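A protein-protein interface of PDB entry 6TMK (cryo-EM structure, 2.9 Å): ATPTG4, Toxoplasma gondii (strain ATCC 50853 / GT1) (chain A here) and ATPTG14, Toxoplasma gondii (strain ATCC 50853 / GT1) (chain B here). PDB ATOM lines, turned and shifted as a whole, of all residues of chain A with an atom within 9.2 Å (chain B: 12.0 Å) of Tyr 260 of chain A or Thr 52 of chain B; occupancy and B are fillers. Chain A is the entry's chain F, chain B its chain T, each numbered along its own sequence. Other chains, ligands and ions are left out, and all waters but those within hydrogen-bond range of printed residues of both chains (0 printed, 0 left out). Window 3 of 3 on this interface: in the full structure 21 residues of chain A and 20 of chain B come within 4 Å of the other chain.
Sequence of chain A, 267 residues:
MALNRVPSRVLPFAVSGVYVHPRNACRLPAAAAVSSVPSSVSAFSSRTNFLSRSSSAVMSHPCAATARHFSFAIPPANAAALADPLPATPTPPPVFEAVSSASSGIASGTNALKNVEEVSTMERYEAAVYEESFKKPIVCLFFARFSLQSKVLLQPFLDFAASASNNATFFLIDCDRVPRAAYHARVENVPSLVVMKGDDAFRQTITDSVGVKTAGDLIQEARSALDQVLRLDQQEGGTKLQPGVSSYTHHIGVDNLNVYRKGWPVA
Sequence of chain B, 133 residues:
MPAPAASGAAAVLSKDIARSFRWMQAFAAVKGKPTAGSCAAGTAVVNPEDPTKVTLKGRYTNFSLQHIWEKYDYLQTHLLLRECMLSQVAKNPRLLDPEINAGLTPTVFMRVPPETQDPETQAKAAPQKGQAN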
ATOM      1  N   GLU A 126      28.383  21.730 -20.309  1.00  0.00           N
ATOM      2  CA  GLU A 126      27.599  22.950 -20.443  1.00  0.00           C
ATOM      3  C   GLU A 126      28.304  24.132 -19.798  1.00  0.00           C
ATOM      4  O   GLU A 126      28.317  25.233 -20.358  1.00  0.00           O
ATOM      5  CB  GLU A 126      26.223  22.744 -19.819  1.00  0.00           C
ATOM      6  CG  GLU A 126      25.299  21.896 -20.657  1.00  0.00           C
ATOM      7  CD  GLU A 126      23.945  21.681 -20.011  1.00  0.00           C
ATOM      8  OE1 GLU A 126      22.937  21.630 -20.746  1.00  0.00           O
ATOM      9  OE2 GLU A 126      23.888  21.567 -18.769  1.00  0.00           O
ATOM     10  N   ARG A 180      24.935  13.616 -24.926  1.00  0.00           N
ATOM     11  CA  ARG A 180      24.317  14.921 -25.095  1.00  0.00           C
ATOM     12  C   ARG A 180      25.323  15.979 -25.517  1.00  0.00           C
ATOM     13  O   ARG A 180      24.937  16.978 -26.134  1.00  0.00           O
ATOM     14  CB  ARG A 180      23.626  15.328 -23.803  1.00  0.00           C
ATOM     15  CG  ARG A 180      22.230  14.787 -23.666  1.00  0.00           C
ATOM     16  CD  ARG A 180      21.475  15.507 -22.582  1.00  0.00           C
ATOM     17  NE  ARG A 180      21.086  16.845 -23.007  1.00  0.00           N
ATOM     18  CZ  ARG A 180      20.801  17.837 -22.177  1.00  0.00           C
ATOM     19  NH1 ARG A 180      20.466  19.018 -22.659  1.00  0.00           N
ATOM     20  NH2 ARG A 180      20.849  17.651 -20.869  1.00  0.00           N
ATOM     21  N   HIS A 250      18.360  27.685 -28.350  1.00  0.00           N
ATOM     22  CA  HIS A 250      18.805  26.982 -27.153  1.00  0.00           C
ATOM     23  C   HIS A 250      19.031  25.503 -27.427  1.00  0.00           C
ATOM     24  O   HIS A 250      18.953  24.673 -26.520  1.00  0.00           O
ATOM     25  CB  HIS A 250      17.810  27.162 -26.009  1.00  0.00           C
ATOM     26  CG  HIS A 250      17.400  28.580 -25.784  1.00  0.00           C
ATOM     27  ND1 HIS A 250      18.306  29.587 -25.535  1.00  0.00           N
ATOM     28  CD2 HIS A 250      16.178  29.163 -25.775  1.00  0.00           C
ATOM     29  CE1 HIS A 250      17.660  30.728 -25.380  1.00  0.00           C
ATOM     30  NE2 HIS A 250      16.368  30.498 -25.521  1.00  0.00           N
ATOM     31  N   ILE A 252      17.196  23.385 -28.923  1.00  0.00           N
ATOM     32  CA  ILE A 252      16.009  22.610 -28.602  1.00  0.00           C
ATOM     33  C   ILE A 252      15.592  21.719 -29.764  1.00  0.00           C
ATOM     34  O   ILE A 252      15.067  20.624 -29.545  1.00  0.00           O
ATOM     35  CB  ILE A 252      14.867  23.538 -28.167  1.00  0.00           C
ATOM     36  CG1 ILE A 252      15.143  24.068 -26.767  1.00  0.00           C
ATOM     37  CG2 ILE A 252      13.550  22.811 -28.206  1.00  0.00           C
ATOM     38  CD1 ILE A 252      14.357  25.274 -26.406  1.00  0.00           C
ATOM     39  N   ASP A 255      18.333  18.951 -29.445  1.00  0.00           N
ATOM     40  CA  ASP A 255      18.098  18.116 -28.274  1.00  0.00           C
ATOM     41  C   ASP A 255      16.953  18.738 -27.491  1.00  0.00           C
ATOM     42  O   ASP A 255      17.135  19.769 -26.838  1.00  0.00           O
ATOM     43  CB  ASP A 255      19.353  18.011 -27.414  1.00  0.00           C
ATOM     44  CG  ASP A 255      19.310  16.843 -26.456  1.00  0.00           C
ATOM     45  OD1 ASP A 255      19.827  15.765 -26.811  1.00  0.00           O
ATOM     46  OD2 ASP A 255      18.760  16.998 -25.349  1.00  0.00           O
ATOM     47  N   ASN A 256      15.775  18.119 -27.561  1.00  0.00           N
ATOM     48  CA  ASN A 256      14.585  18.700 -26.958  1.00  0.00           C
ATOM     49  C   ASN A 256      14.677  18.795 -25.445  1.00  0.00           C
ATOM     50  O   ASN A 256      13.846  19.475 -24.837  1.00  0.00           O
ATOM     51  CB  ASN A 256      13.342  17.888 -27.318  1.00  0.00           C
ATOM     52  CG  ASN A 256      13.074  17.839 -28.800  1.00  0.00           C
ATOM     53  OD1 ASN A 256      12.929  16.769 -29.377  1.00  0.00           O
ATOM     54  ND2 ASN A 256      12.985  18.995 -29.419  1.00  0.00           N
ATOM     55  N   LEU A 257      15.652  18.140 -24.822  1.00  0.00           N
ATOM     56  CA  LEU A 257      15.747  18.151 -23.370  1.00  0.00           C
ATOM     57  C   LEU A 257      16.207  19.485 -22.814  1.00  0.00           C
ATOM     58  O   LEU A 257      16.241  19.641 -21.589  1.00  0.00           O
ATOM     59  CB  LEU A 257      16.692  17.048 -22.904  1.00  0.00           C
ATOM     60  CG  LEU A 257      16.337  15.631 -23.351  1.00  0.00           C
ATOM     61  CD1 LEU A 257      17.380  14.648 -22.879  1.00  0.00           C
ATOM     62  CD2 LEU A 257      14.973  15.230 -22.851  1.00  0.00           C
ATOM     63  N   ASN A 258      16.561  20.446 -23.663  1.00  0.00           N
ATOM     64  CA  ASN A 258      16.924  21.771 -23.183  1.00  0.00           C
ATOM     65  C   ASN A 258      15.720  22.583 -22.733  1.00  0.00           C
ATOM     66  O   ASN A 258      15.900  23.639 -22.117  1.00  0.00           O
ATOM     67  CB  ASN A 258      17.684  22.526 -24.267  1.00  0.00           C
ATOM     68  CG  ASN A 258      19.047  21.939 -24.539  1.00  0.00           C
ATOM     69  OD1 ASN A 258      19.987  22.149 -23.777  1.00  0.00           O
ATOM     70  ND2 ASN A 258      19.163  21.196 -25.622  1.00  0.00           N
ATOM     71  N   VAL A 259      14.500  22.125 -23.021  1.00  0.00           N
ATOM     72  CA  VAL A 259      13.320  22.805 -22.504  1.00  0.00           C
ATOM     73  C   VAL A 259      13.305  22.752 -20.987  1.00  0.00           C
ATOM     74  O   VAL A 259      12.860  23.697 -20.327  1.00  0.00           O
ATOM     75  CB  VAL A 259      12.040  22.185 -23.097  1.00  0.00           C
ATOM     76  CG1 VAL A 259      12.061  22.258 -24.593  1.00  0.00           C
ATOM     77  CG2 VAL A 259      11.887  20.753 -22.652  1.00  0.00           C
ATOM     78  N   TYR A 260      13.788  21.654 -20.407  1.00  0.00           N
ATOM     79  CA  TYR A 260      13.888  21.572 -18.956  1.00  0.00           C
ATOM     80  C   TYR A 260      14.874  22.596 -18.419  1.00  0.00           C
ATOM     81  O   TYR A 260      14.598  23.279 -17.428  1.00  0.00           O
ATOM     82  CB  TYR A 260      14.310  20.169 -18.542  1.00  0.00           C
ATOM     83  CG  TYR A 260      13.290  19.104 -18.827  1.00  0.00           C
ATOM     84  CD1 TYR A 260      12.186  18.939 -18.013  1.00  0.00           C
ATOM     85  CD2 TYR A 260      13.437  18.253 -19.904  1.00  0.00           C
ATOM     86  CE1 TYR A 260      11.255  17.964 -18.273  1.00  0.00           C
ATOM     87  CE2 TYR A 260      12.512  17.277 -20.168  1.00  0.00           C
ATOM     88  CZ  TYR A 260      11.425  17.135 -19.350  1.00  0.00           C
ATOM     89  OH  TYR A 260      10.503  16.158 -19.619  1.00  0.00           O
ATOM     90  N   ARG A 261      16.033  22.715 -19.066  1.00  0.00           N
ATOM     91  CA  ARG A 261      17.002  23.727 -18.675  1.00  0.00           C
ATOM     92  C   ARG A 261      16.393  25.119 -18.725  1.00  0.00           C
ATOM     93  O   ARG A 261      16.581  25.925 -17.806  1.00  0.00           O
ATOM     94  CB  ARG A 261      18.214  23.659 -19.598  1.00  0.00           C
ATOM     95  CG  ARG A 261      19.365  24.524 -19.182  1.00  0.00           C
ATOM     96  CD  ARG A 261      20.466  24.455 -20.207  1.00  0.00           C
ATOM     97  NE  ARG A 261      20.125  25.205 -21.408  1.00  0.00           N
ATOM     98  CZ  ARG A 261      20.741  25.072 -22.574  1.00  0.00           C
ATOM     99  NH1 ARG A 261      21.731  24.206 -22.715  1.00  0.00           N
ATOM    100  NH2 ARG A 261      20.362  25.808 -23.603  1.00  0.00           N
ATOM    101  N   LYS A 262      15.661  25.420 -19.796  1.00  0.00           N
ATOM    102  CA  LYS A 262      15.006  26.713 -19.925  1.00  0.00           C
ATOM    103  C   LYS A 262      13.800  26.863 -19.013  1.00  0.00           C
ATOM    104  O   LYS A 262      13.278  27.973 -18.887  1.00  0.00           O
ATOM    105  CB  LYS A 262      14.583  26.937 -21.371  1.00  0.00           C
ATOM    106  CG  LYS A 262      15.726  26.969 -22.354  1.00  0.00           C
ATOM    107  CD  LYS A 262      16.756  28.025 -22.013  1.00  0.00           C
ATOM    108  CE  LYS A 262      16.152  29.408 -21.969  1.00  0.00           C
ATOM    109  NZ  LYS A 262      17.199  30.461 -21.854  1.00  0.00           N
ATOM    110  N   GLY A 263      13.348  25.784 -18.385  1.00  0.00           N
ATOM    111  CA  GLY A 263      12.241  25.861 -17.464  1.00  0.00           C
ATOM    112  C   GLY A 263      10.881  25.881 -18.107  1.00  0.00           C
ATOM    113  O   GLY A 263       9.895  26.182 -17.425  1.00  0.00           O
ATOM    114  N   TRP A 264      10.788  25.570 -19.392  1.00  0.00           N
ATOM    115  CA  TRP A 264       9.500  25.575 -20.045  1.00  0.00           C
ATOM    116  C   TRP A 264       8.694  24.360 -19.596  1.00  0.00           C
ATOM    117  O   TRP A 264       9.264  23.333 -19.221  1.00  0.00           O
ATOM    118  CB  TRP A 264       9.672  25.548 -21.556  1.00  0.00           C
ATOM    119  CG  TRP A 264      10.316  26.761 -22.113  1.00  0.00           C
ATOM    120  CD1 TRP A 264      10.731  27.853 -21.428  1.00  0.00           C
ATOM    121  CD2 TRP A 264      10.618  27.010 -23.485  1.00  0.00           C
ATOM    122  NE1 TRP A 264      11.279  28.769 -22.282  1.00  0.00           N
ATOM    123  CE2 TRP A 264      11.222  28.273 -23.555  1.00  0.00           C
ATOM    124  CE3 TRP A 264      10.438  26.285 -24.661  1.00  0.00           C
ATOM    125  CZ2 TRP A 264      11.641  28.828 -24.750  1.00  0.00           C
ATOM    126  CZ3 TRP A 264      10.856  26.837 -25.840  1.00  0.00           C
ATOM    127  CH2 TRP A 264      11.449  28.093 -25.880  1.00  0.00           C
ATOM    128  N   PRO A 265       7.370  24.445 -19.627  1.00  0.00           N
ATOM    129  CA  PRO A 265       6.556  23.283 -19.268  1.00  0.00           C
ATOM    130  C   PRO A 265       6.705  22.172 -20.293  1.00  0.00           C
ATOM    131  O   PRO A 265       7.242  22.352 -21.386  1.00  0.00           O
ATOM    132  CB  PRO A 265       5.134  23.843 -19.230  1.00  0.00           C
ATOM    133  CG  PRO A 265       5.165  25.033 -20.091  1.00  0.00           C
ATOM    134  CD  PRO A 265       6.541  25.602 -19.995  1.00  0.00           C
ATOM    135  N   VAL A 266       6.233  20.992 -19.907  1.00  0.00           N
ATOM    136  CA  VAL A 266       6.200  19.847 -20.807  1.00  0.00           C
ATOM    137  C   VAL A 266       4.838  19.176 -20.717  1.00  0.00           C
ATOM    138  O   VAL A 266       4.613  18.118 -21.313  1.00  0.00           O
ATOM    139  CB  VAL A 266       7.323  18.853 -20.478  1.00  0.00           C
ATOM    140  CG1 VAL A 266       8.647  19.395 -20.951  1.00  0.00           C
ATOM    141  CG2 VAL A 266       7.357  18.573 -18.992  1.00  0.00           C
ATOM    142  N   ALA A 267       3.924  19.785 -19.973  1.00  0.00           N
ATOM    143  CA  ALA A 267       2.597  19.223 -19.780  1.00  0.00           C
ATOM    144  C   ALA A 267       1.813  19.238 -21.089  1.00  0.00           C
ATOM    145  O   ALA A 267       1.752  18.240 -21.808  1.00  0.00           O
ATOM    146  CB  ALA A 267       1.854  19.992 -18.703  1.00  0.00           C
ATOM    147  OXT ALA A 267       1.228  20.253 -21.463  1.00  0.00           O
ATOM    148  N   THR B  43      17.189   6.957 -22.874  1.00  0.00           N
ATOM    149  CA  THR B  43      15.934   7.311 -22.232  1.00  0.00           C
ATOM    150  C   THR B  43      16.215   8.430 -21.244  1.00  0.00           C
ATOM    151  O   THR B  43      17.265   8.449 -20.599  1.00  0.00           O
ATOM    152  CB  THR B  43      15.302   6.109 -21.520  1.00  0.00           C
ATOM    153  OG1 THR B  43      13.958   6.425 -21.139  1.00  0.00           O
ATOM    154  CG2 THR B  43      16.085   5.755 -20.282  1.00  0.00           C
ATOM    155  N   ALA B  44      15.271   9.353 -21.132  1.00  0.00           N
ATOM    156  CA  ALA B  44      15.403  10.504 -20.257  1.00  0.00           C
ATOM    157  C   ALA B  44      14.743  10.238 -18.916  1.00  0.00           C
ATOM    158  O   ALA B  44      13.694   9.591 -18.842  1.00  0.00           O
ATOM    159  CB  ALA B  44      14.787  11.740 -20.900  1.00  0.00           C
ATOM    160  N   VAL B  45      15.366  10.744 -17.856  1.00  0.00           N
ATOM    161  CA  VAL B  45      14.826  10.675 -16.506  1.00  0.00           C
ATOM    162  C   VAL B  45      14.958  12.056 -15.888  1.00  0.00           C
ATOM    163  O   VAL B  45      16.062  12.609 -15.818  1.00  0.00           O
ATOM    164  CB  VAL B  45      15.539   9.617 -15.648  1.00  0.00           C
ATOM    165  CG1 VAL B  45      15.167   8.230 -16.109  1.00  0.00           C
ATOM    166  CG2 VAL B  45      17.042   9.800 -15.714  1.00  0.00           C
ATOM    167  N   VAL B  46      13.839  12.612 -15.455  1.00  0.00           N
ATOM    168  CA  VAL B  46      13.804  13.944 -14.871  1.00  0.00           C
ATOM    169  C   VAL B  46      13.909  13.811 -13.362  1.00  0.00           C
ATOM    170  O   VAL B  46      13.216  12.987 -12.753  1.00  0.00           O
ATOM    171  CB  VAL B  46      12.520  14.682 -15.273  1.00  0.00           C
ATOM    172  CG1 VAL B  46      12.625  16.142 -14.932  1.00  0.00           C
ATOM    173  CG2 VAL B  46      12.254  14.503 -16.747  1.00  0.00           C
ATOM    174  N   ASN B  47      14.770  14.610 -12.755  1.00  0.00           N
ATOM    175  CA  ASN B  47      14.874  14.603 -11.308  1.00  0.00           C
ATOM    176  C   ASN B  47      13.567  15.118 -10.725  1.00  0.00           C
ATOM    177  O   ASN B  47      13.204  16.273 -10.978  1.00  0.00           O
ATOM    178  CB  ASN B  47      16.044  15.462 -10.857  1.00  0.00           C
ATOM    179  CG  ASN B  47      16.250  15.424  -9.363  1.00  0.00           C
ATOM    180  OD1 ASN B  47      15.720  14.555  -8.673  1.00  0.00           O
ATOM    181  ND2 ASN B  47      17.029  16.366  -8.853  1.00  0.00           N
ATOM    182  N   PRO B  48      12.827  14.317  -9.953  1.00  0.00           N
ATOM    183  CA  PRO B  48      11.512  14.784  -9.495  1.00  0.00           C
ATOM    184  C   PRO B  48      11.595  15.961  -8.546  1.00  0.00           C
ATOM    185  O   PRO B  48      10.690  16.805  -8.544  1.00  0.00           O
ATOM    186  CB  PRO B  48      10.909  13.551  -8.806  1.00  0.00           C
ATOM    187  CG  PRO B  48      11.812  12.410  -9.134  1.00  0.00           C
ATOM    188  CD  PRO B  48      13.149  12.986  -9.414  1.00  0.00           C
ATOM    189  N   GLU B  49      12.653  16.048  -7.738  1.00  0.00           N
ATOM    190  CA  GLU B  49      12.781  17.169  -6.819  1.00  0.00           C
ATOM    191  C   GLU B  49      13.170  18.447  -7.548  1.00  0.00           C
ATOM    192  O   GLU B  49      12.812  19.544  -7.107  1.00  0.00           O
ATOM    193  CB  GLU B  49      13.815  16.831  -5.753  1.00  0.00           C
ATOM    194  CG  GLU B  49      13.392  15.696  -4.847  1.00  0.00           C
ATOM    195  CD  GLU B  49      14.466  15.316  -3.850  1.00  0.00           C
ATOM    196  OE1 GLU B  49      15.588  15.852  -3.952  1.00  0.00           O
ATOM    197  OE2 GLU B  49      14.189  14.479  -2.965  1.00  0.00           O
ATOM    198  N   ASP B  50      13.901  18.326  -8.653  1.00  0.00           N
ATOM    199  CA  ASP B  50      14.323  19.469  -9.460  1.00  0.00           C
ATOM    200  C   ASP B  50      13.978  19.159 -10.909  1.00  0.00           C
ATOM    201  O   ASP B  50      14.794  18.583 -11.641  1.00  0.00           O
ATOM    202  CB  ASP B  50      15.811  19.753  -9.290  1.00  0.00           C
ATOM    203  CG  ASP B  50      16.217  21.088  -9.873  1.00  0.00           C
ATOM    204  OD1 ASP B  50      15.344  21.780 -10.438  1.00  0.00           O
ATOM    205  OD2 ASP B  50      17.408  21.448  -9.766  1.00  0.00           O
ATOM    206  N   PRO B  51      12.775  19.523 -11.364  1.00  0.00           N
ATOM    207  CA  PRO B  51      12.373  19.157 -12.728  1.00  0.00           C
ATOM    208  C   PRO B  51      13.179  19.853 -13.804  1.00  0.00           C
ATOM    209  O   PRO B  51      13.105  19.445 -14.970  1.00  0.00           O
ATOM    210  CB  PRO B  51      10.903  19.572 -12.771  1.00  0.00           C
ATOM    211  CG  PRO B  51      10.842  20.732 -11.846  1.00  0.00           C
ATOM    212  CD  PRO B  51      11.755  20.356 -10.711  1.00  0.00           C
ATOM    213  N   THR B  52      13.941  20.889 -13.456  1.00  0.00           N
ATOM    214  CA  THR B  52      14.851  21.502 -14.411  1.00  0.00           C
ATOM    215  C   THR B  52      16.015  20.583 -14.749  1.00  0.00           C
ATOM    216  O   THR B  52      16.652  20.763 -15.792  1.00  0.00           O
ATOM    217  CB  THR B  52      15.364  22.832 -13.860  1.00  0.00           C
ATOM    218  OG1 THR B  52      14.293  23.782 -13.831  1.00  0.00           O
ATOM    219  CG2 THR B  52      16.487  23.381 -14.710  1.00  0.00           C
ATOM    220  N   LYS B  53      16.301  19.606 -13.896  1.00  0.00           N
ATOM    221  CA  LYS B  53      17.431  18.708 -14.071  1.00  0.00           C
ATOM    222  C   LYS B  53      16.955  17.410 -14.710  1.00  0.00           C
ATOM    223  O   LYS B  53      15.963  16.817 -14.270  1.00  0.00           O
ATOM    224  CB  LYS B  53      18.114  18.432 -12.733  1.00  0.00           C
ATOM    225  CG  LYS B  53      18.602  19.684 -12.026  1.00  0.00           C
ATOM    226  CD  LYS B  53      19.814  20.282 -12.716  1.00  0.00           C
ATOM    227  CE  LYS B  53      20.160  21.647 -12.149  1.00  0.00           C
ATOM    228  NZ  LYS B  53      20.904  21.558 -10.867  1.00  0.00           N
ATOM    229  N   VAL B  54      17.675  16.969 -15.734  1.00  0.00           N
ATOM    230  CA  VAL B  54      17.258  15.841 -16.556  1.00  0.00           C
ATOM    231  C   VAL B  54      18.504  15.108 -17.019  1.00  0.00           C
ATOM    232  O   VAL B  54      19.482  15.728 -17.445  1.00  0.00           O
ATOM    233  CB  VAL B  54      16.401  16.309 -17.751  1.00  0.00           C
ATOM    234  CG1 VAL B  54      17.166  17.309 -18.590  1.00  0.00           C
ATOM    235  CG2 VAL B  54      15.969  15.133 -18.586  1.00  0.00           C
ATOM    236  N   THR B  55      18.466  13.783 -16.931  1.00  0.00           N
ATOM    237  CA  THR B  55      19.598  12.943 -17.274  1.00  0.00           C
ATOM    238  C   THR B  55      19.215  12.006 -18.409  1.00  0.00           C
ATOM    239  O   THR B  55      18.071  11.553 -18.508  1.00  0.00           O
ATOM    240  CB  THR B  55      20.069  12.130 -16.067  1.00  0.00           C
ATOM    241  OG1 THR B  55      20.377  13.018 -14.987  1.00  0.00           O
ATOM    242  CG2 THR B  55      21.311  11.336 -16.414  1.00  0.00           C
ATOM    243  N   LEU B  56      20.183  11.728 -19.270  1.00  0.00           N
ATOM    244  CA  LEU B  56      20.008  10.838 -20.409  1.00  0.00           C
ATOM    245  C   LEU B  56      20.787   9.556 -20.146  1.00  0.00           C
ATOM    246  O   LEU B  56      22.021   9.549 -20.208  1.00  0.00           O
ATOM    247  CB  LEU B  56      20.478  11.516 -21.690  1.00  0.00           C
ATOM    248  CG  LEU B  56      20.306  10.738 -22.984  1.00  0.00           C
ATOM    249  CD1 LEU B  56      18.849  10.527 -23.285  1.00  0.00           C
ATOM    250  CD2 LEU B  56      20.966  11.490 -24.097  1.00  0.00           C
ATOM    251  N   LYS B  57      20.069   8.478 -19.846  1.00  0.00           N
ATOM    252  CA  LYS B  57      20.675   7.174 -19.632  1.00  0.00           C
ATOM    253  C   LYS B  57      20.742   6.430 -20.958  1.00  0.00           C
ATOM    254  O   LYS B  57      19.713   6.223 -21.608  1.00  0.00           O
ATOM    255  CB  LYS B  57      19.871   6.370 -18.613  1.00  0.00           C
ATOM    256  CG  LYS B  57      19.592   7.103 -17.313  1.00  0.00           C
ATOM    257  CD  LYS B  57      20.860   7.395 -16.534  1.00  0.00           C
ATOM    258  CE  LYS B  57      21.468   6.134 -15.955  1.00  0.00           C
ATOM    259  NZ  LYS B  57      22.591   6.453 -15.036  1.00  0.00           N
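The guanidinium group (NH1) of Arg 261 of chain A sits at hydrogen-bond distance from the side-chain amide oxygen (OD1) of Asn 258 of chain A (2.9 Å).
The backbone NH (N) of Thr 52 of chain B lies close to the side-chain carboxylate (OD1) of Asp 50 of chain B, at 3.4 Å.
The guanidinium group of Arg 261 of chain A lies within salt-bridge range of the side-chain carboxylate of Glu 126 of chain A (3.5 Å).
The backbone carbonyl oxygen (O) of His 250 of chain A lies within hydrogen-bond range of the guanidinium group (NH2) of Arg 261 of chain A.
NH1 of Arg 180 of chain A sits at hydrogen-bond distance from OD1 of Asn 258 of chain A, at 3.4 Å.
The side-chain carboxylate of Asp 255 of chain A sits close to the backbone NH of Leu 257 of chain A.
Among the printed residues, merely in contact across the chains: Tyr 260 of chain A with Pro 51 of chain B (3.2 Å), Tyr 260 of chain A with Thr 52 of chain B (3.3 Å), Arg 180 of chain A with Leu 56 of chain B (3.6 Å), Tyr 260 of chain A with Val 46 of chain B (3.7 Å), Arg 261 of chain A with Thr 52 of chain B (3.9 Å) and Leu 257 of chain A with Val 54 of chain B (3.9 Å).
No residue of chain B comes within 4 Å of Val 259 of chain A.
Of the printed residues of chain B, Tyr 260 of chain A touches Val 46 (3.7 Å), Pro 51 (3.2 Å) and Thr 52 (3.3 Å).
Of the printed residues of chain B, Arg 261 of chain A touches Thr 52.
Gly 263 of chain A touches none of the printed residues of chain B.
No residue of chain B comes within 4 Å of Val 266 of chain A.
Of the printed residues of chain A, Val 46 of chain B touches Tyr 260.
Of chain A, only Tyr 260 (3.2 Å) comes within 4 Å of Pro 51 of chain B.
Of chain A, only Tyr 260 and Arg 261 come within 4 Å of Thr 52 of chain B.
Printed residues of chain A within 4 Å of Val 54 of chain B: Leu 257.
The nearest residue of chain A that does not touch Thr 52 of chain B is Gly 263 of chain A (4.7 Å).
The nearest printed residue of chain A that does not touch Val 46 of chain B is Leu 257 of chain A (6.7 Å).
Printed residues of chain A that touch a printed residue of chain B: Arg 180, Leu 257, Tyr 260 and Arg 261.
Hydrophobic or aromatic side chains of chain A that line the printed part of chain B: Tyr 260.
Along chain A the printed residues that touch a printed residue of chain B span positions 180 to 261.
Of the 15 printed residues of chain B, 5 touch a printed residue of chain A.
Hydrophobic or aromatic side chains of chain B that line the printed part of chain A: Val 46, Val 54 and Leu 56.
Along chain B the printed residues that touch a printed residue of chain A span positions 46 to 56.
Among the printed residues, no Asp or Glu carboxylate lies within 4 Å of a Lys or Arg side-chain nitrogen of the other chain.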
